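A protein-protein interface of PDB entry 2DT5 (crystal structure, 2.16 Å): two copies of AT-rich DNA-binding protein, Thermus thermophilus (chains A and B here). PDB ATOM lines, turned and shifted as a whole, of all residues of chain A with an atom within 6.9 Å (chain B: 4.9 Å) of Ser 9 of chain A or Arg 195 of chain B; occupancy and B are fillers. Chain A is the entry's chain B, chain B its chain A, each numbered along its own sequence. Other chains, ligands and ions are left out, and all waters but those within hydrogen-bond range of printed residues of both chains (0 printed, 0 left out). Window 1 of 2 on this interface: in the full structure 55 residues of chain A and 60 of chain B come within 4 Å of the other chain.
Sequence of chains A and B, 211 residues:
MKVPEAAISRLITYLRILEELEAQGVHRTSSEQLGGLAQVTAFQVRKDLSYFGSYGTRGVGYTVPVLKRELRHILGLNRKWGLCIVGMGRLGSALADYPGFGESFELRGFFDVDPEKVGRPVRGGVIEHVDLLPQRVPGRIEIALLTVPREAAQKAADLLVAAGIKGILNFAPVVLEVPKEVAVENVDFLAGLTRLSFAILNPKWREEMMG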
ATOM      1  N   PRO A   4       1.164 -23.106 -32.267  1.00  0.00           N
ATOM      2  CA  PRO A   4       0.466 -21.818 -32.367  1.00  0.00           C
ATOM      3  C   PRO A   4       1.298 -20.839 -33.174  1.00  0.00           C
ATOM      4  O   PRO A   4       2.518 -20.998 -33.289  1.00  0.00           O
ATOM      5  CB  PRO A   4       0.325 -21.384 -30.913  1.00  0.00           C
ATOM      6  CG  PRO A   4       1.597 -21.913 -30.301  1.00  0.00           C
ATOM      7  CD  PRO A   4       1.701 -23.311 -30.908  1.00  0.00           C
ATOM      8  N   GLU A   5       0.635 -19.842 -33.744  1.00  0.00           N
ATOM      9  CA  GLU A   5       1.318 -18.820 -34.529  1.00  0.00           C
ATOM     10  C   GLU A   5       2.458 -18.259 -33.684  1.00  0.00           C
ATOM     11  O   GLU A   5       2.252 -17.909 -32.519  1.00  0.00           O
ATOM     12  CB  GLU A   5       0.327 -17.728 -34.907  1.00  0.00           C
ATOM     13  CG  GLU A   5       0.910 -16.567 -35.686  1.00  0.00           C
ATOM     14  CD  GLU A   5      -0.189 -15.718 -36.285  1.00  0.00           C
ATOM     15  OE1 GLU A   5      -0.691 -16.100 -37.363  1.00  0.00           O
ATOM     16  OE2 GLU A   5      -0.565 -14.692 -35.668  1.00  0.00           O
ATOM     17  N   ALA A   6       3.649 -18.169 -34.278  1.00  0.00           N
ATOM     18  CA  ALA A   6       4.839 -17.725 -33.558  1.00  0.00           C
ATOM     19  C   ALA A   6       5.480 -16.400 -33.952  1.00  0.00           C
ATOM     20  O   ALA A   6       6.220 -15.819 -33.152  1.00  0.00           O
ATOM     21  CB  ALA A   6       5.901 -18.822 -33.627  1.00  0.00           C
ATOM     22  N   ALA A   7       5.221 -15.936 -35.174  1.00  0.00           N
ATOM     23  CA  ALA A   7       5.812 -14.691 -35.650  1.00  0.00           C
ATOM     24  C   ALA A   7       5.612 -13.540 -34.690  1.00  0.00           C
ATOM     25  O   ALA A   7       6.566 -12.827 -34.381  1.00  0.00           O
ATOM     26  CB  ALA A   7       5.255 -14.319 -37.040  1.00  0.00           C
ATOM     27  N   ILE A   8       4.383 -13.346 -34.209  1.00  0.00           N
ATOM     28  CA  ILE A   8       4.147 -12.246 -33.283  1.00  0.00           C
ATOM     29  C   ILE A   8       4.886 -12.465 -31.960  1.00  0.00           C
ATOM     30  O   ILE A   8       5.356 -11.507 -31.334  1.00  0.00           O
ATOM     31  CB  ILE A   8       2.645 -12.019 -33.029  1.00  0.00           C
ATOM     32  CG1 ILE A   8       1.903 -11.909 -34.365  1.00  0.00           C
ATOM     33  CG2 ILE A   8       2.452 -10.714 -32.267  1.00  0.00           C
ATOM     34  CD1 ILE A   8       2.457 -10.804 -35.285  1.00  0.00           C
ATOM     35  N   SER A   9       5.005 -13.720 -31.539  1.00  0.00           N
ATOM     36  CA  SER A   9       5.737 -14.039 -30.304  1.00  0.00           C
ATOM     37  C   SER A   9       7.205 -13.641 -30.500  1.00  0.00           C
ATOM     38  O   SER A   9       7.840 -13.107 -29.593  1.00  0.00           O
ATOM     39  CB  SER A   9       5.630 -15.541 -29.983  1.00  0.00           C
ATOM     40  OG  SER A   9       4.291 -15.894 -29.649  1.00  0.00           O
ATOM     41  N   ARG A  10       7.745 -13.890 -31.688  1.00  0.00           N
ATOM     42  CA  ARG A  10       9.129 -13.496 -31.945  1.00  0.00           C
ATOM     43  C   ARG A  10       9.296 -11.971 -31.837  1.00  0.00           C
ATOM     44  O   ARG A  10      10.256 -11.482 -31.236  1.00  0.00           O
ATOM     45  CB  ARG A  10       9.573 -13.969 -33.323  1.00  0.00           C
ATOM     46  CG  ARG A  10       9.817 -15.470 -33.397  1.00  0.00           C
ATOM     47  CD  ARG A  10      10.788 -15.802 -34.539  1.00  0.00           C
ATOM     48  NE  ARG A  10      10.262 -15.450 -35.856  1.00  0.00           N
ATOM     49  CZ  ARG A  10       9.279 -16.108 -36.462  1.00  0.00           C
ATOM     50  NH1 ARG A  10       8.710 -17.157 -35.868  1.00  0.00           N
ATOM     51  NH2 ARG A  10       8.877 -15.730 -37.669  1.00  0.00           N
ATOM     52  N   LEU A  11       8.355 -11.221 -32.399  1.00  0.00           N
ATOM     53  CA  LEU A  11       8.442  -9.768 -32.325  1.00  0.00           C
ATOM     54  C   LEU A  11       8.429  -9.320 -30.861  1.00  0.00           C
ATOM     55  O   LEU A  11       9.193  -8.427 -30.460  1.00  0.00           O
ATOM     56  CB  LEU A  11       7.285  -9.110 -33.087  1.00  0.00           C
ATOM     57  CG  LEU A  11       7.245  -9.341 -34.605  1.00  0.00           C
ATOM     58  CD1 LEU A  11       6.124  -8.500 -35.212  1.00  0.00           C
ATOM     59  CD2 LEU A  11       8.578  -8.950 -35.227  1.00  0.00           C
ATOM     60  N   ILE A  12       7.560  -9.947 -30.070  1.00  0.00           N
ATOM     61  CA  ILE A  12       7.453  -9.644 -28.649  1.00  0.00           C
ATOM     62  C   ILE A  12       8.793  -9.964 -27.979  1.00  0.00           C
ATOM     63  O   ILE A  12       9.269  -9.211 -27.131  1.00  0.00           O
ATOM     64  CB  ILE A  12       6.291 -10.450 -28.001  1.00  0.00           C
ATOM     65  CG1 ILE A  12       4.957  -9.975 -28.604  1.00  0.00           C
ATOM     66  CG2 ILE A  12       6.287 -10.262 -26.458  1.00  0.00           C
ATOM     67  CD1 ILE A  12       3.748 -10.896 -28.347  1.00  0.00           C
ATOM     68  N   THR A  13       9.420 -11.060 -28.382  1.00  0.00           N
ATOM     69  CA  THR A  13      10.724 -11.408 -27.810  1.00  0.00           C
ATOM     70  C   THR A  13      11.770 -10.331 -28.128  1.00  0.00           C
ATOM     71  O   THR A  13      12.522  -9.899 -27.244  1.00  0.00           O
ATOM     72  CB  THR A  13      11.233 -12.735 -28.365  1.00  0.00           C
ATOM     73  OG1 THR A  13      10.338 -13.787 -27.985  1.00  0.00           O
ATOM     74  CG2 THR A  13      12.623 -13.024 -27.836  1.00  0.00           C
ATOM     75  N   TYR A  14      11.807  -9.900 -29.392  1.00  0.00           N
ATOM     76  CA  TYR A  14      12.759  -8.887 -29.832  1.00  0.00           C
ATOM     77  C   TYR A  14      12.568  -7.611 -29.028  1.00  0.00           C
ATOM     78  O   TYR A  14      13.536  -6.913 -28.693  1.00  0.00           O
ATOM     79  CB  TYR A  14      12.549  -8.568 -31.321  1.00  0.00           C
ATOM     80  CG  TYR A  14      12.671  -9.750 -32.263  1.00  0.00           C
ATOM     81  CD1 TYR A  14      11.964  -9.772 -33.466  1.00  0.00           C
ATOM     82  CD2 TYR A  14      13.514 -10.823 -31.974  1.00  0.00           C
ATOM     83  CE1 TYR A  14      12.085 -10.831 -34.368  1.00  0.00           C
ATOM     84  CE2 TYR A  14      13.649 -11.896 -32.876  1.00  0.00           C
ATOM     85  CZ  TYR A  14      12.923 -11.890 -34.072  1.00  0.00           C
ATOM     86  OH  TYR A  14      12.998 -12.934 -34.959  1.00  0.00           O
ATOM     87  N   LEU A  15      11.313  -7.304 -28.721  1.00  0.00           N
ATOM     88  CA  LEU A  15      11.008  -6.101 -27.969  1.00  0.00           C
ATOM     89  C   LEU A  15      11.542  -6.192 -26.537  1.00  0.00           C
ATOM     90  O   LEU A  15      12.088  -5.208 -26.014  1.00  0.00           O
ATOM     91  CB  LEU A  15       9.506  -5.841 -27.971  1.00  0.00           C
ATOM     92  CG  LEU A  15       9.082  -4.594 -27.200  1.00  0.00           C
ATOM     93  CD1 LEU A  15       9.754  -3.366 -27.809  1.00  0.00           C
ATOM     94  CD2 LEU A  15       7.556  -4.448 -27.226  1.00  0.00           C
ATOM     95  N   LEU A  75       2.838  -3.897 -32.815  1.00  0.00           N
ATOM     96  CA  LEU A  75       2.153  -4.743 -31.853  1.00  0.00           C
ATOM     97  C   LEU A  75       0.919  -4.097 -31.230  1.00  0.00           C
ATOM     98  O   LEU A  75       0.135  -4.772 -30.562  1.00  0.00           O
ATOM     99  CB  LEU A  75       3.154  -5.195 -30.763  1.00  0.00           C
ATOM    100  CG  LEU A  75       4.278  -6.098 -31.310  1.00  0.00           C
ATOM    101  CD1 LEU A  75       5.383  -6.292 -30.260  1.00  0.00           C
ATOM    102  CD2 LEU A  75       3.708  -7.449 -31.726  1.00  0.00           C
ATOM    103  N   PHE A 105      -2.104  -1.214 -21.469  1.00  0.00           N
ATOM    104  CA  PHE A 105      -3.323  -1.894 -21.031  1.00  0.00           C
ATOM    105  C   PHE A 105      -3.868  -1.296 -19.752  1.00  0.00           C
ATOM    106  O   PHE A 105      -3.202  -1.306 -18.722  1.00  0.00           O
ATOM    107  CB  PHE A 105      -3.019  -3.372 -20.824  1.00  0.00           C
ATOM    108  CG  PHE A 105      -2.357  -4.007 -22.002  1.00  0.00           C
ATOM    109  CD1 PHE A 105      -1.011  -4.338 -21.961  1.00  0.00           C
ATOM    110  CD2 PHE A 105      -3.069  -4.234 -23.174  1.00  0.00           C
ATOM    111  CE1 PHE A 105      -0.381  -4.883 -23.059  1.00  0.00           C
ATOM    112  CE2 PHE A 105      -2.442  -4.786 -24.291  1.00  0.00           C
ATOM    113  CZ  PHE A 105      -1.100  -5.110 -24.236  1.00  0.00           C
ATOM    114  N   LEU A 169      -8.596 -12.800 -23.310  1.00  0.00           N
ATOM    115  CA  LEU A 169      -7.436 -13.480 -22.779  1.00  0.00           C
ATOM    116  C   LEU A 169      -8.073 -14.492 -21.831  1.00  0.00           C
ATOM    117  O   LEU A 169      -8.493 -14.160 -20.719  1.00  0.00           O
ATOM    118  CB  LEU A 169      -6.483 -12.551 -22.037  1.00  0.00           C
ATOM    119  CG  LEU A 169      -5.115 -13.105 -21.637  1.00  0.00           C
ATOM    120  CD1 LEU A 169      -4.319 -13.454 -22.887  1.00  0.00           C
ATOM    121  CD2 LEU A 169      -4.352 -12.106 -20.767  1.00  0.00           C
ATOM    122  N   ALA A 183     -10.799 -12.110 -31.315  1.00  0.00           N
ATOM    123  CA  ALA A 183      -9.543 -12.817 -31.077  1.00  0.00           C
ATOM    124  C   ALA A 183      -9.549 -13.493 -29.704  1.00  0.00           C
ATOM    125  O   ALA A 183     -10.184 -13.009 -28.760  1.00  0.00           O
ATOM    126  CB  ALA A 183      -8.367 -11.843 -31.182  1.00  0.00           C
ATOM    127  N   GLU A 185      -6.879 -15.766 -26.918  1.00  0.00           N
ATOM    128  CA  GLU A 185      -5.567 -16.275 -26.511  1.00  0.00           C
ATOM    129  C   GLU A 185      -5.790 -16.945 -25.174  1.00  0.00           C
ATOM    130  O   GLU A 185      -6.353 -16.336 -24.259  1.00  0.00           O
ATOM    131  CB  GLU A 185      -4.560 -15.137 -26.330  1.00  0.00           C
ATOM    132  CG  GLU A 185      -4.082 -14.525 -27.634  1.00  0.00           C
ATOM    133  CD  GLU A 185      -3.056 -15.411 -28.343  1.00  0.00           C
ATOM    134  OE1 GLU A 185      -3.083 -15.478 -29.595  1.00  0.00           O
ATOM    135  OE2 GLU A 185      -2.217 -16.023 -27.640  1.00  0.00           O
ATOM    136  N   ASN A 186      -5.375 -18.202 -25.076  1.00  0.00           N
ATOM    137  CA  ASN A 186      -5.513 -18.968 -23.847  1.00  0.00           C
ATOM    138  C   ASN A 186      -4.218 -18.899 -23.054  1.00  0.00           C
ATOM    139  O   ASN A 186      -3.122 -19.003 -23.613  1.00  0.00           O
ATOM    140  CB  ASN A 186      -5.841 -20.418 -24.175  1.00  0.00           C
ATOM    141  CG  ASN A 186      -7.084 -20.536 -25.018  1.00  0.00           C
ATOM    142  OD1 ASN A 186      -8.140 -20.059 -24.634  1.00  0.00           O
ATOM    143  ND2 ASN A 186      -6.957 -21.151 -26.184  1.00  0.00           N
ATOM    144  N   ALA B 191       2.652 -11.433 -23.027  1.00  0.00           N
ATOM    145  CA  ALA B 191       2.841 -11.823 -24.422  1.00  0.00           C
ATOM    146  C   ALA B 191       1.483 -12.183 -25.032  1.00  0.00           C
ATOM    147  O   ALA B 191       1.199 -11.852 -26.185  1.00  0.00           O
ATOM    148  CB  ALA B 191       3.810 -13.004 -24.526  1.00  0.00           C
ATOM    149  N   GLY B 192       0.646 -12.854 -24.253  1.00  0.00           N
ATOM    150  CA  GLY B 192      -0.675 -13.225 -24.736  1.00  0.00           C
ATOM    151  C   GLY B 192      -1.515 -11.976 -24.996  1.00  0.00           C
ATOM    152  O   GLY B 192      -2.233 -11.904 -25.997  1.00  0.00           O
ATOM    153  N   LEU B 193      -1.427 -11.000 -24.093  1.00  0.00           N
ATOM    154  CA  LEU B 193      -2.164  -9.750 -24.237  1.00  0.00           C
ATOM    155  C   LEU B 193      -1.711  -9.014 -25.483  1.00  0.00           C
ATOM    156  O   LEU B 193      -2.513  -8.379 -26.169  1.00  0.00           O
ATOM    157  CB  LEU B 193      -1.908  -8.833 -23.048  1.00  0.00           C
ATOM    158  CG  LEU B 193      -3.000  -8.654 -22.014  1.00  0.00           C
ATOM    159  CD1 LEU B 193      -2.523  -7.572 -21.041  1.00  0.00           C
ATOM    160  CD2 LEU B 193      -4.326  -8.249 -22.690  1.00  0.00           C
ATOM    161  N   THR B 194      -0.413  -9.081 -25.750  1.00  0.00           N
ATOM    162  CA  THR B 194       0.153  -8.403 -26.900  1.00  0.00           C
ATOM    163  C   THR B 194      -0.269  -9.095 -28.189  1.00  0.00           C
ATOM    164  O   THR B 194      -0.593  -8.413 -29.170  1.00  0.00           O
ATOM    165  CB  THR B 194       1.678  -8.326 -26.765  1.00  0.00           C
ATOM    166  OG1 THR B 194       1.981  -7.623 -25.552  1.00  0.00           O
ATOM    167  CG2 THR B 194       2.298  -7.554 -27.944  1.00  0.00           C
ATOM    168  N   ARG B 195      -0.275 -10.434 -28.198  1.00  0.00           N
ATOM    169  CA  ARG B 195      -0.726 -11.148 -29.383  1.00  0.00           C
ATOM    170  C   ARG B 195      -2.209 -10.772 -29.634  1.00  0.00           C
ATOM    171  O   ARG B 195      -2.629 -10.660 -30.786  1.00  0.00           O
ATOM    172  CB  ARG B 195      -0.574 -12.668 -29.231  1.00  0.00           C
ATOM    173  CG  ARG B 195       0.870 -13.165 -29.386  1.00  0.00           C
ATOM    174  CD  ARG B 195       0.962 -14.685 -29.456  1.00  0.00           C
ATOM    175  NE  ARG B 195       0.517 -15.344 -28.228  1.00  0.00           N
ATOM    176  CZ  ARG B 195       1.299 -15.595 -27.175  1.00  0.00           C
ATOM    177  NH1 ARG B 195       2.587 -15.250 -27.175  1.00  0.00           N
ATOM    178  NH2 ARG B 195       0.794 -16.200 -26.110  1.00  0.00           N
ATOM    179  N   LEU B 196      -2.992 -10.554 -28.574  1.00  0.00           N
ATOM    180  CA  LEU B 196      -4.406 -10.165 -28.760  1.00  0.00           C
ATOM    181  C   LEU B 196      -4.457  -8.782 -29.405  1.00  0.00           C
ATOM    182  O   LEU B 196      -5.227  -8.544 -30.331  1.00  0.00           O
ATOM    183  CB  LEU B 196      -5.156 -10.093 -27.432  1.00  0.00           C
ATOM    184  CG  LEU B 196      -5.897 -11.303 -26.876  1.00  0.00           C
ATOM    185  CD1 LEU B 196      -6.646 -10.841 -25.625  1.00  0.00           C
ATOM    186  CD2 LEU B 196      -6.890 -11.871 -27.909  1.00  0.00           C
ATOM    187  N   SER B 197      -3.633  -7.880 -28.887  1.00  0.00           N
ATOM    188  CA  SER B 197      -3.538  -6.526 -29.395  1.00  0.00           C
ATOM    189  C   SER B 197      -3.262  -6.566 -30.892  1.00  0.00           C
ATOM    190  O   SER B 197      -3.952  -5.921 -31.673  1.00  0.00           O
ATOM    191  CB  SER B 197      -2.401  -5.785 -28.696  1.00  0.00           C
ATOM    192  OG  SER B 197      -2.145  -4.551 -29.327  1.00  0.00           O
ATOM    193  N   PHE B 198      -2.253  -7.326 -31.288  1.00  0.00           N
ATOM    194  CA  PHE B 198      -1.914  -7.398 -32.692  1.00  0.00           C
ATOM    195  C   PHE B 198      -3.060  -7.972 -33.520  1.00  0.00           C
ATOM    196  O   PHE B 198      -3.374  -7.449 -34.594  1.00  0.00           O
ATOM    197  CB  PHE B 198      -0.662  -8.253 -32.921  1.00  0.00           C
ATOM    198  CG  PHE B 198      -0.321  -8.433 -34.378  1.00  0.00           C
ATOM    199  CD1 PHE B 198       0.439  -7.476 -35.058  1.00  0.00           C
ATOM    200  CD2 PHE B 198      -0.839  -9.510 -35.092  1.00  0.00           C
ATOM    201  CE1 PHE B 198       0.672  -7.591 -36.428  1.00  0.00           C
ATOM    202  CE2 PHE B 198      -0.616  -9.642 -36.468  1.00  0.00           C
ATOM    203  CZ  PHE B 198       0.143  -8.674 -37.140  1.00  0.00           C
ATOM    204  N   ALA B 199      -3.675  -9.039 -33.016  1.00  0.00           N
ATOM    205  CA  ALA B 199      -4.767  -9.712 -33.713  1.00  0.00           C
ATOM    206  C   ALA B 199      -6.001  -8.828 -33.907  1.00  0.00           C
ATOM    207  O   ALA B 199      -6.643  -8.865 -34.960  1.00  0.00           O
ATOM    208  CB  ALA B 199      -5.145 -11.001 -32.967  1.00  0.00           C
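No position is printed for both chains.
OG of Ser 9 of chain A lies within hydrogen-bond range of NH1 of Arg 195 of chain B (3.1 Å). OE2 of Glu 185 of chain A lies within salt-bridge range of NE of Arg 195 of chain B, 2.9 Å away. OG of Ser 197 of chain B lies within hydrogen-bond range of O of Leu 75 of chain A, 2.6 Å away.
Among the printed residues, pairs that only touch across the chains: Ile 12 of chain A with Ala 191 of chain B (3.5 Å), Ile 8 of chain A with Phe 198 of chain B (3.5 Å), Leu 75 of chain A with Phe 198 of chain B (3.6 Å), Ala 183 of chain A with Leu 196 of chain B (3.6 Å), Glu 185 of chain A with Gly 192 of chain B (3.6 Å), Leu 169 of chain A with Leu 196 of chain B (3.6 Å), Ile 12 of chain A with Thr 194 of chain B (3.7 Å), Phe 105 of chain A with Leu 193 of chain B (3.7 Å), Leu 75 of chain A with Thr 194 of chain B (3.8 Å), Glu 185 of chain A with Leu 196 of chain B (3.8 Å), Ala 183 of chain A with Ala 199 of chain B (3.8 Å), Leu 169 of chain A with Gly 192 of chain B (3.8 Å), Ile 12 of chain A with Arg 195 of chain B (3.8 Å) and Leu 169 of chain A with Leu 193 of chain B (3.9 Å).
Of the 9 printed residues of chain B, 9 touch a printed residue of chain A. Hydrophobic or aromatic side chains of chain B that line the printed part of chain A: Leu 193, Leu 196, Phe 198 and Ala 199. Among the printed residues, Asp or Glu carboxylates within 4 Å of a Lys or Arg side-chain nitrogen of the other chain: Glu 185 of chain A with Arg 195 of chain B.
Of chain B, only Arg 195 comes within 4 Å of Ser 9 of chain A. Arg 195 of chain B touches three residues of chain A. Of the printed residues of chain A, Phe 198 of chain B touches Ile 8 (3.5 Å) and Leu 75 (3.6 Å). Of the printed residues of chain B, Ile 12 of chain A touches Ala 191 (3.5 Å), Thr 194 (3.7 Å) and Arg 195 (3.8 Å). The nearest printed residue of chain B that does not touch Ser 9 of chain A is Ala 191 of chain B (5.9 Å). The nearest residue of chain A that does not touch Arg 195 of chain B is Ile 8 of chain A (4.1 Å). The nearest printed residue of chain B that does not touch Ile 8 of chain A is Arg 195 of chain B (4.1 Å).
O of Ser 9 of chain A lies within hydrogen-bond range of OG1 of Thr 13 of chain A, 3.0 Å away.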
